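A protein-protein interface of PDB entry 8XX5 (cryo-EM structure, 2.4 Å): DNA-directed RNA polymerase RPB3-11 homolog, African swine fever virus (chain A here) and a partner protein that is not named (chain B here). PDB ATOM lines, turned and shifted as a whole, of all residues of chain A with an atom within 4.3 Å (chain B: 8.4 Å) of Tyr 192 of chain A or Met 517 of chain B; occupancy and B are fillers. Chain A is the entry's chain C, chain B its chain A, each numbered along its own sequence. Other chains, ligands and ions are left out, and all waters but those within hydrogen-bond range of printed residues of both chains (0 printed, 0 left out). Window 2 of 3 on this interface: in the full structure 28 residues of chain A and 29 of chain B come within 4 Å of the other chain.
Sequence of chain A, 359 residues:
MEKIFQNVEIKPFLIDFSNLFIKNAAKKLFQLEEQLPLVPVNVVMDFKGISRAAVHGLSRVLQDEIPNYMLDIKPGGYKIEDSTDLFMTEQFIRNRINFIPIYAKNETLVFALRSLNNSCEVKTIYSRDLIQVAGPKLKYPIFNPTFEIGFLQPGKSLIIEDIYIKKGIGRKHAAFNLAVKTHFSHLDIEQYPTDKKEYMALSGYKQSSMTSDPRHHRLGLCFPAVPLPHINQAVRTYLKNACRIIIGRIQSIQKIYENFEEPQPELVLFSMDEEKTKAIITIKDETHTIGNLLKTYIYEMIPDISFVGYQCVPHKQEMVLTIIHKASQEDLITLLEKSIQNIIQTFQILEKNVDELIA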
ATOM      1  N   GLN A 191       6.992   6.951 -32.168  1.00  0.00           N
ATOM      2  CA  GLN A 191       8.332   6.448 -32.427  1.00  0.00           C
ATOM      3  C   GLN A 191       9.270   6.805 -31.283  1.00  0.00           C
ATOM      4  O   GLN A 191       9.153   7.875 -30.678  1.00  0.00           O
ATOM      5  CB  GLN A 191       8.884   7.007 -33.742  1.00  0.00           C
ATOM      6  CG  GLN A 191       8.071   6.630 -34.965  1.00  0.00           C
ATOM      7  CD  GLN A 191       8.934   6.410 -36.189  1.00  0.00           C
ATOM      8  OE1 GLN A 191      10.019   5.839 -36.103  1.00  0.00           O
ATOM      9  NE2 GLN A 191       8.454   6.861 -37.339  1.00  0.00           N
ATOM     10  N   TYR A 192      10.195   5.899 -30.990  1.00  0.00           N
ATOM     11  CA  TYR A 192      11.255   6.144 -30.030  1.00  0.00           C
ATOM     12  C   TYR A 192      12.362   6.981 -30.658  1.00  0.00           C
ATOM     13  O   TYR A 192      12.507   7.020 -31.882  1.00  0.00           O
ATOM     14  CB  TYR A 192      11.843   4.824 -29.543  1.00  0.00           C
ATOM     15  CG  TYR A 192      11.043   4.127 -28.474  1.00  0.00           C
ATOM     16  CD1 TYR A 192      10.576   4.816 -27.366  1.00  0.00           C
ATOM     17  CD2 TYR A 192      10.766   2.772 -28.568  1.00  0.00           C
ATOM     18  CE1 TYR A 192       9.847   4.176 -26.386  1.00  0.00           C
ATOM     19  CE2 TYR A 192      10.039   2.125 -27.595  1.00  0.00           C
ATOM     20  CZ  TYR A 192       9.582   2.829 -26.506  1.00  0.00           C
ATOM     21  OH  TYR A 192       8.855   2.183 -25.532  1.00  0.00           O
ATOM     22  N   PRO A 193      13.161   7.664 -29.841  1.00  0.00           N
ATOM     23  CA  PRO A 193      14.415   8.227 -30.356  1.00  0.00           C
ATOM     24  C   PRO A 193      15.451   7.131 -30.550  1.00  0.00           C
ATOM     25  O   PRO A 193      16.021   6.630 -29.577  1.00  0.00           O
ATOM     26  CB  PRO A 193      14.836   9.222 -29.266  1.00  0.00           C
ATOM     27  CG  PRO A 193      13.626   9.400 -28.394  1.00  0.00           C
ATOM     28  CD  PRO A 193      12.881   8.112 -28.469  1.00  0.00           C
ATOM     29  N   THR A 194      15.703   6.752 -31.800  1.00  0.00           N
ATOM     30  CA  THR A 194      16.593   5.640 -32.106  1.00  0.00           C
ATOM     31  C   THR A 194      18.058   6.047 -32.151  1.00  0.00           C
ATOM     32  O   THR A 194      18.918   5.188 -32.373  1.00  0.00           O
ATOM     33  CB  THR A 194      16.199   4.996 -33.438  1.00  0.00           C
ATOM     34  OG1 THR A 194      16.289   5.966 -34.489  1.00  0.00           O
ATOM     35  CG2 THR A 194      14.782   4.458 -33.367  1.00  0.00           C
ATOM     36  N   TYR A 199      17.553   2.395 -27.618  1.00  0.00           N
ATOM     37  CA  TYR A 199      16.556   2.103 -28.641  1.00  0.00           C
ATOM     38  C   TYR A 199      17.157   1.844 -30.014  1.00  0.00           C
ATOM     39  O   TYR A 199      16.406   1.693 -30.983  1.00  0.00           O
ATOM     40  CB  TYR A 199      15.543   3.248 -28.735  1.00  0.00           C
ATOM     41  CG  TYR A 199      14.932   3.640 -27.412  1.00  0.00           C
ATOM     42  CD1 TYR A 199      14.236   2.717 -26.646  1.00  0.00           C
ATOM     43  CD2 TYR A 199      15.043   4.936 -26.933  1.00  0.00           C
ATOM     44  CE1 TYR A 199      13.674   3.072 -25.438  1.00  0.00           C
ATOM     45  CE2 TYR A 199      14.484   5.301 -25.728  1.00  0.00           C
ATOM     46  CZ  TYR A 199      13.801   4.366 -24.984  1.00  0.00           C
ATOM     47  OH  TYR A 199      13.242   4.726 -23.781  1.00  0.00           O
ATOM     48  N   GLY A 204      11.834   1.284 -33.572  1.00  0.00           N
ATOM     49  CA  GLY A 204      11.579   2.685 -33.317  1.00  0.00           C
ATOM     50  C   GLY A 204      10.144   2.946 -32.919  1.00  0.00           C
ATOM     51  O   GLY A 204       9.881   3.776 -32.046  1.00  0.00           O
ATOM     52  N   TYR A 205       9.208   2.233 -33.540  1.00  0.00           N
ATOM     53  CA  TYR A 205       7.804   2.370 -33.182  1.00  0.00           C
ATOM     54  C   TYR A 205       7.583   1.942 -31.739  1.00  0.00           C
ATOM     55  O   TYR A 205       8.213   1.001 -31.253  1.00  0.00           O
ATOM     56  CB  TYR A 205       6.930   1.537 -34.117  1.00  0.00           C
ATOM     57  CG  TYR A 205       6.856   2.089 -35.515  1.00  0.00           C
ATOM     58  CD1 TYR A 205       6.465   3.400 -35.740  1.00  0.00           C
ATOM     59  CD2 TYR A 205       7.179   1.302 -36.609  1.00  0.00           C
ATOM     60  CE1 TYR A 205       6.397   3.911 -37.017  1.00  0.00           C
ATOM     61  CE2 TYR A 205       7.111   1.804 -37.887  1.00  0.00           C
ATOM     62  CZ  TYR A 205       6.721   3.110 -38.085  1.00  0.00           C
ATOM     63  OH  TYR A 205       6.656   3.615 -39.359  1.00  0.00           O
ATOM     64  N   LYS A 206       6.684   2.646 -31.054  1.00  0.00           N
ATOM     65  CA  LYS A 206       6.417   2.392 -29.644  1.00  0.00           C
ATOM     66  C   LYS A 206       5.425   1.259 -29.417  1.00  0.00           C
ATOM     67  O   LYS A 206       5.163   0.914 -28.259  1.00  0.00           O
ATOM     68  CB  LYS A 206       5.918   3.669 -28.967  1.00  0.00           C
ATOM     69  CG  LYS A 206       6.991   4.734 -28.818  1.00  0.00           C
ATOM     70  CD  LYS A 206       6.698   5.661 -27.655  1.00  0.00           C
ATOM     71  CE  LYS A 206       7.531   6.927 -27.742  1.00  0.00           C
ATOM     72  NZ  LYS A 206       6.745   8.086 -28.241  1.00  0.00           N
ATOM     73  N   GLN A 207       4.880   0.667 -30.475  1.00  0.00           N
ATOM     74  CA  GLN A 207       4.007  -0.493 -30.371  1.00  0.00           C
ATOM     75  C   GLN A 207       4.623  -1.666 -31.118  1.00  0.00           C
ATOM     76  O   GLN A 207       5.266  -1.484 -32.156  1.00  0.00           O
ATOM     77  CB  GLN A 207       2.613  -0.199 -30.931  1.00  0.00           C
ATOM     78  CG  GLN A 207       2.091   1.187 -30.614  1.00  0.00           C
ATOM     79  CD  GLN A 207       0.675   1.401 -31.108  1.00  0.00           C
ATOM     80  OE1 GLN A 207      -0.090   0.451 -31.266  1.00  0.00           O
ATOM     81  NE2 GLN A 207       0.318   2.656 -31.352  1.00  0.00           N
ATOM     82  N   SER A 208       4.430  -2.866 -30.582  1.00  0.00           N
ATOM     83  CA  SER A 208       4.846  -4.074 -31.278  1.00  0.00           C
ATOM     84  C   SER A 208       3.982  -4.297 -32.511  1.00  0.00           C
ATOM     85  O   SER A 208       2.773  -4.060 -32.490  1.00  0.00           O
ATOM     86  CB  SER A 208       4.753  -5.282 -30.349  1.00  0.00           C
ATOM     87  OG  SER A 208       5.537  -6.357 -30.829  1.00  0.00           O
ATOM     88  N   ARG B 512       9.412 -16.627 -24.867  1.00  0.00           N
ATOM     89  CA  ARG B 512       9.913 -15.794 -23.783  1.00  0.00           C
ATOM     90  C   ARG B 512       8.792 -14.940 -23.201  1.00  0.00           C
ATOM     91  O   ARG B 512       7.856 -14.543 -23.898  1.00  0.00           O
ATOM     92  CB  ARG B 512      11.060 -14.907 -24.267  1.00  0.00           C
ATOM     93  CG  ARG B 512      10.686 -13.946 -25.368  1.00  0.00           C
ATOM     94  CD  ARG B 512      11.871 -13.106 -25.791  1.00  0.00           C
ATOM     95  NE  ARG B 512      11.549 -12.270 -26.941  1.00  0.00           N
ATOM     96  CZ  ARG B 512      12.306 -11.275 -27.380  1.00  0.00           C
ATOM     97  NH1 ARG B 512      13.445 -10.961 -26.787  1.00  0.00           N
ATOM     98  NH2 ARG B 512      11.911 -10.583 -28.443  1.00  0.00           N
ATOM     99  N   ASN B 514       8.887 -11.831 -21.783  1.00  0.00           N
ATOM    100  CA  ASN B 514       8.920 -10.412 -22.092  1.00  0.00           C
ATOM    101  C   ASN B 514       9.824 -10.153 -23.285  1.00  0.00           C
ATOM    102  O   ASN B 514      10.823 -10.844 -23.496  1.00  0.00           O
ATOM    103  CB  ASN B 514       9.415  -9.587 -20.895  1.00  0.00           C
ATOM    104  CG  ASN B 514       8.471  -9.646 -19.717  1.00  0.00           C
ATOM    105  OD1 ASN B 514       8.848 -10.076 -18.629  1.00  0.00           O
ATOM    106  ND2 ASN B 514       7.237  -9.205 -19.922  1.00  0.00           N
ATOM    107  N   THR B 515       9.453  -9.152 -24.062  1.00  0.00           N
ATOM    108  CA  THR B 515      10.276  -8.566 -25.099  1.00  0.00           C
ATOM    109  C   THR B 515      10.780  -7.210 -24.631  1.00  0.00           C
ATOM    110  O   THR B 515      10.351  -6.701 -23.591  1.00  0.00           O
ATOM    111  CB  THR B 515       9.471  -8.414 -26.398  1.00  0.00           C
ATOM    112  OG1 THR B 515       8.431  -7.446 -26.213  1.00  0.00           O
ATOM    113  CG2 THR B 515       8.857  -9.740 -26.805  1.00  0.00           C
ATOM    114  N   PRO B 516      11.706  -6.593 -25.367  1.00  0.00           N
ATOM    115  CA  PRO B 516      12.031  -5.187 -25.077  1.00  0.00           C
ATOM    116  C   PRO B 516      10.828  -4.269 -25.186  1.00  0.00           C
ATOM    117  O   PRO B 516      10.881  -3.138 -24.691  1.00  0.00           O
ATOM    118  CB  PRO B 516      13.101  -4.844 -26.126  1.00  0.00           C
ATOM    119  CG  PRO B 516      13.114  -5.998 -27.092  1.00  0.00           C
ATOM    120  CD  PRO B 516      12.661  -7.182 -26.319  1.00  0.00           C
ATOM    121  N   MET B 517       9.747  -4.726 -25.812  1.00  0.00           N
ATOM    122  CA  MET B 517       8.542  -3.939 -26.020  1.00  0.00           C
ATOM    123  C   MET B 517       7.489  -4.159 -24.941  1.00  0.00           C
ATOM    124  O   MET B 517       6.393  -3.598 -25.040  1.00  0.00           O
ATOM    125  CB  MET B 517       7.944  -4.269 -27.388  1.00  0.00           C
ATOM    126  CG  MET B 517       7.272  -3.092 -28.015  1.00  0.00           C
ATOM    127  SD  MET B 517       8.511  -2.243 -28.989  1.00  0.00           S
ATOM    128  CE  MET B 517       8.054  -0.567 -28.638  1.00  0.00           C
ATOM    129  N   GLY B 518       7.787  -4.961 -23.918  1.00  0.00           N
ATOM    130  CA  GLY B 518       6.822  -5.310 -22.897  1.00  0.00           C
ATOM    131  C   GLY B 518       6.558  -6.805 -22.875  1.00  0.00           C
ATOM    132  O   GLY B 518       7.427  -7.610 -23.232  1.00  0.00           O
ATOM    133  N   LYS B 519       5.352  -7.167 -22.448  1.00  0.00           N
ATOM    134  CA  LYS B 519       4.964  -8.570 -22.425  1.00  0.00           C
ATOM    135  C   LYS B 519       4.887  -9.122 -23.841  1.00  0.00           C
ATOM    136  O   LYS B 519       4.378  -8.468 -24.755  1.00  0.00           O
ATOM    137  CB  LYS B 519       3.623  -8.745 -21.716  1.00  0.00           C
ATOM    138  CG  LYS B 519       3.716  -9.492 -20.394  1.00  0.00           C
ATOM    139  CD  LYS B 519       2.343  -9.851 -19.849  1.00  0.00           C
ATOM    140  CE  LYS B 519       1.515 -10.620 -20.866  1.00  0.00           C
ATOM    141  NZ  LYS B 519       1.954 -12.034 -21.012  1.00  0.00           N
ATOM    142  N   ASN B 520       5.403 -10.335 -24.020  1.00  0.00           N
ATOM    143  CA  ASN B 520       5.436 -10.990 -25.326  1.00  0.00           C
ATOM    144  C   ASN B 520       4.038 -11.504 -25.643  1.00  0.00           C
ATOM    145  O   ASN B 520       3.682 -12.640 -25.327  1.00  0.00           O
ATOM    146  CB  ASN B 520       6.462 -12.114 -25.333  1.00  0.00           C
ATOM    147  CG  ASN B 520       6.810 -12.580 -26.729  1.00  0.00           C
ATOM    148  OD1 ASN B 520       6.365 -12.004 -27.720  1.00  0.00           O
ATOM    149  ND2 ASN B 520       7.611 -13.635 -26.815  1.00  0.00           N
ATOM    150  N   VAL B 521       3.233 -10.651 -26.275  1.00  0.00           N
ATOM    151  CA  VAL B 521       1.871 -10.994 -26.652  1.00  0.00           C
ATOM    152  C   VAL B 521       1.622 -10.543 -28.083  1.00  0.00           C
ATOM    153  O   VAL B 521       2.289  -9.648 -28.606  1.00  0.00           O
ATOM    154  CB  VAL B 521       0.821 -10.367 -25.709  1.00  0.00           C
ATOM    155  CG1 VAL B 521       0.777 -11.114 -24.391  1.00  0.00           C
ATOM    156  CG2 VAL B 521       1.118  -8.896 -25.487  1.00  0.00           C
ATOM    157  N   GLU B 726      18.462  -9.184 -23.826  1.00  0.00           N
ATOM    158  CA  GLU B 726      17.140  -9.208 -24.432  1.00  0.00           C
ATOM    159  C   GLU B 726      17.137  -8.659 -25.850  1.00  0.00           C
ATOM    160  O   GLU B 726      16.100  -8.717 -26.519  1.00  0.00           O
ATOM    161  CB  GLU B 726      16.149  -8.424 -23.564  1.00  0.00           C
ATOM    162  CG  GLU B 726      16.156  -6.924 -23.796  1.00  0.00           C
ATOM    163  CD  GLU B 726      15.061  -6.212 -23.024  1.00  0.00           C
ATOM    164  OE1 GLU B 726      13.984  -6.814 -22.829  1.00  0.00           O
ATOM    165  OE2 GLU B 726      15.275  -5.051 -22.616  1.00  0.00           O
ATOM    166  N   THR B 727      18.267  -8.139 -26.325  1.00  0.00           N
ATOM    167  CA  THR B 727      18.327  -7.488 -27.627  1.00  0.00           C
ATOM    168  C   THR B 727      19.513  -7.975 -28.454  1.00  0.00           C
ATOM    169  O   THR B 727      19.487  -7.896 -29.685  1.00  0.00           O
ATOM    170  CB  THR B 727      18.374  -5.967 -27.433  1.00  0.00           C
ATOM    171  OG1 THR B 727      17.306  -5.352 -28.167  1.00  0.00           O
ATOM    172  CG2 THR B 727      19.714  -5.382 -27.870  1.00  0.00           C
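The backbone carbonyl oxygen (O) of Gln 191 of chain A is in hydrogen-bond range of the side-chain amino group (NZ) of Lys 206 of chain A (3.4 Å).
The side-chain hydroxyl of Thr 515 of chain B sits close to the backbone NH of Met 517 of chain B (3.0 Å).
Among the printed residues, pairs that only touch across the chains: Tyr 192 of chain A with Met 517 of chain B (3.5 Å), Tyr 205 of chain A with Met 517 of chain B (3.1 Å), Lys 206 of chain A with Met 517 of chain B (3.3 Å), Gln 207 of chain A with Met 517 of chain B (3.9 Å) and Ser 208 of chain A with Met 517 of chain B (3.8 Å).
Tyr 192 of chain A touches just one residue of chain B: Met 517.
No residue of chain B comes within 4 Å of Pro 193 of chain A.
Of the printed residues of chain B, Ser 208 of chain A touches Met 517.
Printed residues of chain B within 4 Å of Tyr 205 of chain A: Met 517 (3.1 Å).
Of the printed residues of chain B, Gln 207 of chain A touches Met 517 (3.9 Å).
Printed residues of chain B within 4 Å of Lys 206 of chain A: Met 517.
Asn 514 of chain B touches none of the printed residues of chain A.
Thr 515 of chain B touches none of the printed residues of chain A.
The nearest printed residue of chain A that does not touch Met 517 of chain B is Gly 204 of chain A (5.8 Å).
The nearest printed residue of chain B that does not touch Tyr 205 of chain A is Pro 516 of chain B (8.2 Å).
Hydrophobic or aromatic side chains of chain B that line the printed part of chain A: Met 517.
Among the printed residues, 5 pairs touch across the chains.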
